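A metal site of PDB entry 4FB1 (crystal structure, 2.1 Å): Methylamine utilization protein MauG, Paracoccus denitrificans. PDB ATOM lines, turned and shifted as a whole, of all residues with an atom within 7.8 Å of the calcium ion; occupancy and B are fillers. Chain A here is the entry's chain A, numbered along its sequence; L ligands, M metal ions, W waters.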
ATOM      1  N   ARG A  39     -19.410 -27.323 -29.708  1.00  0.00           N
ATOM      2  CA  ARG A  39     -19.184 -26.139 -28.902  1.00  0.00           C
ATOM      3  C   ARG A  39     -19.604 -26.318 -27.462  1.00  0.00           C
ATOM      4  O   ARG A  39     -20.318 -25.520 -26.929  1.00  0.00           O
ATOM      5  CB  ARG A  39     -19.895 -24.944 -29.473  1.00  0.00           C
ATOM      6  CG  ARG A  39     -19.248 -23.683 -29.073  1.00  0.00           C
ATOM      7  CD  ARG A  39     -20.089 -22.534 -29.418  1.00  0.00           C
ATOM      8  NE  ARG A  39     -19.343 -21.294 -29.365  1.00  0.00           N
ATOM      9  CZ  ARG A  39     -19.528 -20.344 -28.481  1.00  0.00           C
ATOM     10  NH1 ARG A  39     -20.416 -20.482 -27.522  1.00  0.00           N
ATOM     11  NH2 ARG A  39     -18.809 -19.247 -28.532  1.00  0.00           N
ATOM     12  N   THR A  42     -23.205 -25.637 -26.607  1.00  0.00           N
ATOM     13  CA  THR A  42     -23.752 -24.272 -26.595  1.00  0.00           C
ATOM     14  C   THR A  42     -23.928 -23.877 -28.053  1.00  0.00           C
ATOM     15  O   THR A  42     -23.622 -24.672 -28.953  1.00  0.00           O
ATOM     16  CB  THR A  42     -22.837 -23.260 -25.850  1.00  0.00           C
ATOM     17  OG1 THR A  42     -21.525 -23.251 -26.430  1.00  0.00           O
ATOM     18  CG2 THR A  42     -22.713 -23.628 -24.381  1.00  0.00           C
ATOM     19  N   ASP A  43     -24.422 -22.651 -28.254  1.00  0.00           N
ATOM     20  CA  ASP A  43     -24.869 -22.204 -29.550  1.00  0.00           C
ATOM     21  C   ASP A  43     -23.808 -21.410 -30.315  1.00  0.00           C
ATOM     22  O   ASP A  43     -23.526 -20.212 -29.985  1.00  0.00           O
ATOM     23  CB  ASP A  43     -26.207 -21.454 -29.491  1.00  0.00           C
ATOM     24  CG  ASP A  43     -26.933 -21.415 -30.872  1.00  0.00           C
ATOM     25  OD1 ASP A  43     -28.129 -20.973 -30.941  1.00  0.00           O
ATOM     26  OD2 ASP A  43     -26.311 -21.828 -31.904  1.00  0.00           O
ATOM     27  N   LEU A  51     -24.134 -13.852 -30.206  1.00  0.00           N
ATOM     28  CA  LEU A  51     -24.201 -15.171 -29.589  1.00  0.00           C
ATOM     29  C   LEU A  51     -24.821 -15.123 -28.186  1.00  0.00           C
ATOM     30  O   LEU A  51     -24.817 -16.162 -27.483  1.00  0.00           O
ATOM     31  CB  LEU A  51     -22.790 -15.784 -29.492  1.00  0.00           C
ATOM     32  CG  LEU A  51     -22.223 -16.635 -30.639  1.00  0.00           C
ATOM     33  CD1 LEU A  51     -22.813 -16.314 -32.011  1.00  0.00           C
ATOM     34  CD2 LEU A  51     -20.677 -16.545 -30.671  1.00  0.00           C
ATOM     35  N   ALA A  52     -25.341 -13.940 -27.808  1.00  0.00           N
ATOM     36  CA  ALA A  52     -25.937 -13.673 -26.490  1.00  0.00           C
ATOM     37  C   ALA A  52     -27.112 -14.574 -26.271  1.00  0.00           C
ATOM     38  O   ALA A  52     -27.266 -15.168 -25.184  1.00  0.00           O
ATOM     39  CB  ALA A  52     -26.355 -12.209 -26.337  1.00  0.00           C
ATOM     40  N   ASN A  66     -28.799 -16.632 -22.505  1.00  0.00           N
ATOM     41  CA  ASN A  66     -27.700 -17.398 -23.122  1.00  0.00           C
ATOM     42  C   ASN A  66     -27.895 -18.907 -22.904  1.00  0.00           C
ATOM     43  O   ASN A  66     -28.274 -19.423 -21.770  1.00  0.00           O
ATOM     44  CB  ASN A  66     -26.372 -16.898 -22.539  1.00  0.00           C
ATOM     45  CG  ASN A  66     -25.158 -17.469 -23.202  1.00  0.00           C
ATOM     46  OD1 ASN A  66     -24.336 -18.131 -22.517  1.00  0.00           O
ATOM     47  ND2 ASN A  66     -24.978 -17.213 -24.563  1.00  0.00           N
ATOM     48  N   THR A  67     -27.712 -19.617 -24.010  1.00  0.00           N
ATOM     49  CA  THR A  67     -27.849 -21.054 -23.998  1.00  0.00           C
ATOM     50  C   THR A  67     -26.623 -21.630 -23.247  1.00  0.00           C
ATOM     51  O   THR A  67     -25.456 -21.412 -23.621  1.00  0.00           O
ATOM     52  CB  THR A  67     -27.981 -21.571 -25.441  1.00  0.00           C
ATOM     53  OG1 THR A  67     -29.186 -21.076 -26.019  1.00  0.00           O
ATOM     54  CG2 THR A  67     -27.956 -23.104 -25.479  1.00  0.00           C
ATOM     55  N   PRO A  68     -26.885 -22.297 -22.119  1.00  0.00           N
ATOM     56  CA  PRO A  68     -25.788 -22.789 -21.321  1.00  0.00           C
ATOM     57  C   PRO A  68     -25.275 -24.167 -21.835  1.00  0.00           C
ATOM     58  O   PRO A  68     -25.960 -24.896 -22.578  1.00  0.00           O
ATOM     59  CB  PRO A  68     -26.408 -22.911 -19.906  1.00  0.00           C
ATOM     60  CG  PRO A  68     -27.825 -23.253 -20.185  1.00  0.00           C
ATOM     61  CD  PRO A  68     -28.190 -22.587 -21.496  1.00  0.00           C
ATOM     62  N   THR A  69     -24.075 -24.534 -21.393  1.00  0.00           N
ATOM     63  CA  THR A  69     -23.548 -25.849 -21.686  1.00  0.00           C
ATOM     64  C   THR A  69     -24.414 -26.914 -21.045  1.00  0.00           C
ATOM     65  O   THR A  69     -24.997 -26.659 -19.997  1.00  0.00           O
ATOM     66  CB  THR A  69     -22.162 -25.998 -21.084  1.00  0.00           C
ATOM     67  OG1 THR A  69     -21.637 -27.244 -21.520  1.00  0.00           O
ATOM     68  CG2 THR A  69     -22.236 -25.953 -19.494  1.00  0.00           C
ATOM     69  N   TRP A  93     -31.350 -21.199 -15.827  1.00  0.00           N
ATOM     70  CA  TRP A  93     -30.602 -20.216 -15.079  1.00  0.00           C
ATOM     71  C   TRP A  93     -31.365 -19.725 -13.847  1.00  0.00           C
ATOM     72  O   TRP A  93     -30.790 -19.030 -13.001  1.00  0.00           O
ATOM     73  CB  TRP A  93     -30.311 -19.023 -15.954  1.00  0.00           C
ATOM     74  CG  TRP A  93     -29.266 -19.174 -16.958  1.00  0.00           C
ATOM     75  CD1 TRP A  93     -29.456 -19.393 -18.320  1.00  0.00           C
ATOM     76  CD2 TRP A  93     -27.870 -18.951 -16.776  1.00  0.00           C
ATOM     77  NE1 TRP A  93     -28.241 -19.348 -18.972  1.00  0.00           N
ATOM     78  CE2 TRP A  93     -27.252 -19.078 -18.051  1.00  0.00           C
ATOM     79  CE3 TRP A  93     -27.072 -18.625 -15.660  1.00  0.00           C
ATOM     80  CZ2 TRP A  93     -25.865 -18.929 -18.229  1.00  0.00           C
ATOM     81  CZ3 TRP A  93     -25.688 -18.451 -15.842  1.00  0.00           C
ATOM     82  CH2 TRP A  93     -25.104 -18.607 -17.109  1.00  0.00           C
ATOM     83  N   VAL A 272     -15.770 -23.163 -19.187  1.00  0.00           N
ATOM     84  CA  VAL A 272     -16.123 -21.740 -19.210  1.00  0.00           C
ATOM     85  C   VAL A 272     -15.318 -21.030 -20.277  1.00  0.00           C
ATOM     86  O   VAL A 272     -15.800 -20.066 -20.883  1.00  0.00           O
ATOM     87  CB  VAL A 272     -16.081 -20.993 -17.807  1.00  0.00           C
ATOM     88  CG1 VAL A 272     -14.682 -20.859 -17.255  1.00  0.00           C
ATOM     89  CG2 VAL A 272     -16.786 -19.625 -17.844  1.00  0.00           C
ATOM     90  N   VAL A 274     -14.775 -21.870 -23.245  1.00  0.00           N
ATOM     91  CA  VAL A 274     -15.247 -22.027 -24.606  1.00  0.00           C
ATOM     92  C   VAL A 274     -16.757 -21.794 -24.757  1.00  0.00           C
ATOM     93  O   VAL A 274     -17.318 -21.973 -25.860  1.00  0.00           O
ATOM     94  CB  VAL A 274     -14.823 -23.404 -25.260  1.00  0.00           C
ATOM     95  CG1 VAL A 274     -13.314 -23.618 -25.163  1.00  0.00           C
ATOM     96  CG2 VAL A 274     -15.542 -24.556 -24.644  1.00  0.00           C
ATOM     97  N   THR A 275     -17.428 -21.381 -23.681  1.00  0.00           N
ATOM     98  CA  THR A 275     -18.878 -21.168 -23.811  1.00  0.00           C
ATOM     99  C   THR A 275     -19.307 -19.695 -23.714  1.00  0.00           C
ATOM    100  O   THR A 275     -20.450 -19.406 -23.332  1.00  0.00           O
ATOM    101  CB  THR A 275     -19.591 -21.965 -22.750  1.00  0.00           C
ATOM    102  OG1 THR A 275     -18.941 -21.692 -21.488  1.00  0.00           O
ATOM    103  CG2 THR A 275     -19.438 -23.374 -23.060  1.00  0.00           C
ATOM    104  N   GLY A 276     -18.417 -18.750 -24.037  1.00  0.00           N
ATOM    105  CA  GLY A 276     -18.821 -17.340 -24.148  1.00  0.00           C
ATOM    106  C   GLY A 276     -19.959 -17.136 -25.156  1.00  0.00           C
ATOM    107  O   GLY A 276     -20.265 -18.058 -25.951  1.00  0.00           O
ATOM    108  N   PRO A 277     -20.668 -15.991 -25.087  1.00  0.00           N
ATOM    109  CA  PRO A 277     -20.562 -14.979 -24.067  1.00  0.00           C
ATOM    110  C   PRO A 277     -21.109 -15.453 -22.723  1.00  0.00           C
ATOM    111  O   PRO A 277     -21.608 -16.585 -22.606  1.00  0.00           O
ATOM    112  CB  PRO A 277     -21.382 -13.817 -24.639  1.00  0.00           C
ATOM    113  CG  PRO A 277     -22.357 -14.437 -25.492  1.00  0.00           C
ATOM    114  CD  PRO A 277     -21.749 -15.675 -26.030  1.00  0.00           C
ATOM    115  N   TYR A 278     -20.992 -14.596 -21.719  1.00  0.00           N
ATOM    116  CA  TYR A 278     -21.106 -15.052 -20.359  1.00  0.00           C
ATOM    117  C   TYR A 278     -22.308 -14.444 -19.637  1.00  0.00           C
ATOM    118  O   TYR A 278     -22.974 -13.533 -20.124  1.00  0.00           O
ATOM    119  CB  TYR A 278     -19.770 -14.821 -19.638  1.00  0.00           C
ATOM    120  CG  TYR A 278     -18.666 -15.595 -20.290  1.00  0.00           C
ATOM    121  CD1 TYR A 278     -17.788 -14.983 -21.203  1.00  0.00           C
ATOM    122  CD2 TYR A 278     -18.518 -16.940 -20.057  1.00  0.00           C
ATOM    123  CE1 TYR A 278     -16.810 -15.722 -21.824  1.00  0.00           C
ATOM    124  CE2 TYR A 278     -17.549 -17.646 -20.648  1.00  0.00           C
ATOM    125  CZ  TYR A 278     -16.694 -17.051 -21.514  1.00  0.00           C
ATOM    126  OH  TYR A 278     -15.721 -17.822 -22.096  1.00  0.00           O
ATOM    127  N   MET A 279     -22.588 -15.011 -18.473  1.00  0.00           N
ATOM    128  CA  MET A 279     -23.755 -14.675 -17.686  1.00  0.00           C
ATOM    129  C   MET A 279     -25.033 -15.112 -18.336  1.00  0.00           C
ATOM    130  O   MET A 279     -25.057 -15.428 -19.552  1.00  0.00           O
ATOM    131  CB  MET A 279     -23.756 -13.196 -17.314  1.00  0.00           C
ATOM    132  CG  MET A 279     -22.455 -12.774 -16.648  1.00  0.00           C
ATOM    133  SD  MET A 279     -21.928 -13.791 -15.230  1.00  0.00           S
ATOM    134  CE  MET A 279     -20.292 -13.056 -15.003  1.00  0.00           C
ATOM    135  N   HIS A 280     -26.091 -15.084 -17.560  1.00  0.00           N
ATOM    136  CA  HIS A 280     -27.387 -15.578 -17.963  1.00  0.00           C
ATOM    137  C   HIS A 280     -27.905 -14.901 -19.241  1.00  0.00           C
ATOM    138  O   HIS A 280     -28.800 -15.446 -19.891  1.00  0.00           O
ATOM    139  CB  HIS A 280     -28.389 -15.397 -16.814  1.00  0.00           C
ATOM    140  CG  HIS A 280     -28.711 -13.960 -16.531  1.00  0.00           C
ATOM    141  ND1 HIS A 280     -28.169 -13.252 -15.473  1.00  0.00           N
ATOM    142  CD2 HIS A 280     -29.516 -13.083 -17.191  1.00  0.00           C
ATOM    143  CE1 HIS A 280     -28.650 -12.027 -15.468  1.00  0.00           C
ATOM    144  NE2 HIS A 280     -29.442 -11.887 -16.524  1.00  0.00           N
ATOM    145  N   ASN A 281     -27.352 -13.757 -19.595  1.00  0.00           N
ATOM    146  CA  ASN A 281     -27.839 -13.024 -20.743  1.00  0.00           C
ATOM    147  C   ASN A 281     -26.724 -12.730 -21.746  1.00  0.00           C
ATOM    148  O   ASN A 281     -26.800 -11.772 -22.441  1.00  0.00           O
ATOM    149  CB  ASN A 281     -28.542 -11.717 -20.302  1.00  0.00           C
ATOM    150  CG  ASN A 281     -27.581 -10.767 -19.566  1.00  0.00           C
ATOM    151  OD1 ASN A 281     -26.386 -11.029 -19.451  1.00  0.00           O
ATOM    152  ND2 ASN A 281     -28.117  -9.649 -19.066  1.00  0.00           N
ATOM    153  N   GLY A 282     -25.699 -13.570 -21.781  1.00  0.00           N
ATOM    154  CA  GLY A 282     -24.533 -13.386 -22.614  1.00  0.00           C
ATOM    155  C   GLY A 282     -24.015 -11.980 -22.712  1.00  0.00           C
ATOM    156  O   GLY A 282     -23.523 -11.614 -23.770  1.00  0.00           O
ATOM    157  N   PHE A 284     -21.433 -10.345 -21.560  1.00  0.00           N
ATOM    158  CA  PHE A 284     -19.985 -10.192 -21.697  1.00  0.00           C
ATOM    159  C   PHE A 284     -19.452 -11.188 -22.734  1.00  0.00           C
ATOM    160  O   PHE A 284     -19.667 -12.410 -22.585  1.00  0.00           O
ATOM    161  CB  PHE A 284     -19.308 -10.464 -20.341  1.00  0.00           C
ATOM    162  CG  PHE A 284     -19.816  -9.614 -19.227  1.00  0.00           C
ATOM    163  CD1 PHE A 284     -20.079  -8.263 -19.422  1.00  0.00           C
ATOM    164  CD2 PHE A 284     -19.993 -10.151 -17.953  1.00  0.00           C
ATOM    165  CE1 PHE A 284     -20.515  -7.462 -18.414  1.00  0.00           C
ATOM    166  CE2 PHE A 284     -20.448  -9.338 -16.908  1.00  0.00           C
ATOM    167  CZ  PHE A 284     -20.696  -7.964 -17.152  1.00  0.00           C
HETATM  168 FE1  LIG L   1     -19.086 -16.053 -10.450  1.00  0.00          FE
HETATM  169  C1  LIG L   1     -21.071 -16.344 -13.278  1.00  0.00           C
HETATM  170  C2  LIG L   1     -16.341 -16.537 -12.290  1.00  0.00           C
HETATM  171  C3  LIG L   1     -17.193 -14.834  -7.804  1.00  0.00           C
HETATM  172  C4  LIG L   1     -21.745 -16.472  -8.433  1.00  0.00           C
HETATM  173  N1  LIG L   1     -18.764 -16.380 -12.489  1.00  0.00           N
HETATM  174  C5  LIG L   1     -19.633 -16.445 -13.477  1.00  0.00           C
HETATM  175  C6  LIG L   1     -19.042 -16.566 -14.814  1.00  0.00           C
HETATM  176  C7  LIG L   1     -17.685 -16.618 -14.538  1.00  0.00           C
HETATM  177  C8  LIG L   1     -17.600 -16.497 -13.063  1.00  0.00           C
HETATM  178  C9  LIG L   1     -16.513 -16.773 -15.427  1.00  0.00           C
HETATM  179  C10 LIG L   1     -19.802 -16.673 -16.084  1.00  0.00           C
HETATM  180  C11 LIG L   1     -19.743 -18.177 -16.406  1.00  0.00           C
HETATM  181  C12 LIG L   1     -20.831 -18.608 -17.377  1.00  0.00           C
HETATM  182  O1  LIG L   1     -21.534 -17.691 -17.868  1.00  0.00           O
HETATM  183  O2  LIG L   1     -21.042 -19.855 -17.642  1.00  0.00           O
HETATM  184  N2  LIG L   1     -17.105 -15.729 -10.096  1.00  0.00           N
HETATM  185  C13 LIG L   1     -16.124 -16.006 -10.941  1.00  0.00           C
HETATM  186  C14 LIG L   1     -14.783 -15.712 -10.427  1.00  0.00           C
HETATM  187  C15 LIG L   1     -15.025 -15.233  -9.149  1.00  0.00           C
HETATM  188  C16 LIG L   1     -16.486 -15.256  -9.016  1.00  0.00           C
HETATM  189  C17 LIG L   1     -13.484 -15.931 -11.141  1.00  0.00           C
HETATM  190  C18 LIG L   1     -14.027 -14.743  -8.139  1.00  0.00           C
HETATM  191  C19 LIG L   1     -13.500 -13.476  -8.762  1.00  0.00           C
HETATM  192  N3  LIG L   1     -19.407 -15.733  -8.433  1.00  0.00           N
HETATM  193  C20 LIG L   1     -18.571 -15.249  -7.517  1.00  0.00           C
HETATM  194  C21 LIG L   1     -19.164 -15.112  -6.206  1.00  0.00           C
HETATM  195  C22 LIG L   1     -20.455 -15.576  -6.372  1.00  0.00           C
HETATM  196  C23 LIG L   1     -20.536 -15.941  -7.779  1.00  0.00           C
HETATM  197  C24 LIG L   1     -18.439 -14.563  -5.013  1.00  0.00           C
HETATM  198  C25 LIG L   1     -21.580 -15.722  -5.373  1.00  0.00           C
HETATM  199  C26 LIG L   1     -21.662 -14.531  -4.464  1.00  0.00           C
HETATM  200  N4  LIG L   1     -21.068 -16.376 -10.804  1.00  0.00           N
HETATM  201  C27 LIG L   1     -22.037 -16.402  -9.876  1.00  0.00           C
HETATM  202  C28 LIG L   1     -23.398 -16.431 -10.442  1.00  0.00           C
HETATM  203  C29 LIG L   1     -23.146 -16.400 -11.813  1.00  0.00           C
HETATM  204  C30 LIG L   1     -21.701 -16.370 -11.959  1.00  0.00           C
HETATM  205  C31 LIG L   1     -24.705 -16.451  -9.724  1.00  0.00           C
HETATM  206  C32 LIG L   1     -24.121 -16.313 -12.920  1.00  0.00           C
HETATM  207  C33 LIG L   1     -24.498 -14.857 -12.775  1.00  0.00           C
HETATM  208  C34 LIG L   1     -25.564 -14.529 -13.760  1.00  0.00           C
HETATM  209  O3  LIG L   1     -25.437 -14.905 -14.944  1.00  0.00           O
HETATM  210  O4  LIG L   1     -26.536 -13.905 -13.355  1.00  0.00           O
HETATM  211 CA    CA M   1     -22.370 -18.781 -22.300  1.00  0.00          CA
HETATM  212  O   HOH W   1     -23.162 -20.978 -22.481  1.00  0.00           O
HETATM  213  O   HOH W   2     -20.776 -19.826 -20.745  1.00  0.00           O
HETATM  214  O   HOH W   3     -23.193 -18.045 -20.004  1.00  0.00           O
HETATM  215  O   HOH W   4     -22.497 -19.015 -24.878  1.00  0.00           O
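The calcium ion is bound by the side-chain amide oxygen (OD1) of Asn 66 (2.1 Å). O of Thr 275 binds the calcium ion (2.3 Å). Water W1 is bound to the calcium ion (2.3 Å). The calcium ion is bound by O of Pro 277, at 2.3 Å. The calcium ion is bound by water W2 (2.5 Å). The calcium ion is bound by water W3, at 2.5 Å. The calcium ion is bound by water W4. The calcium ion has seven donor atoms within binding distance.
An oxygen (O4) of the ligand is in hydrogen-bond range of a ring nitrogen (ND1) of His 280 (2.8 Å). An oxygen (O1) of the ligand is in hydrogen-bond range of the backbone NH of Met 279, at 2.9 Å. N of His 280 lies within hydrogen-bond range of O3 of the ligand (2.7 Å).
Within 4 Å of the calcium ion: Asn 66, Thr 275 and Pro 277. Along chain A the residues within 4 Å of the calcium ion span positions 66 to 277. The nearest printed residue that does not touch the calcium ion is Gly 276 (4.1 Å).
Water W2 lies within hydrogen-bond range of the side-chain hydroxyl (OG1) of Thr 275 (2.7 Å) and an oxygen (O2) of the ligand (3.1 Å). Water W4 lies within hydrogen-bond range of O of Gly 276 and ND2 of Asn 66. Water W3 bridges an oxygen (O1) of the ligand and the backbone carbonyl oxygen of Met 279.
N of Asn 66 is in hydrogen-bond range of O of His 280 (2.9 Å). ND2 of Asn 66 lies within hydrogen-bond range of O of Leu 51 (3.1 Å). NE1 of Trp 93 sits at hydrogen-bond distance from O of Asn 66, 2.8 Å away. The side-chain amide nitrogen (ND2) of Asn 66 lies close to the backbone carbonyl oxygen (O) of Ala 52 (3.1 Å).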
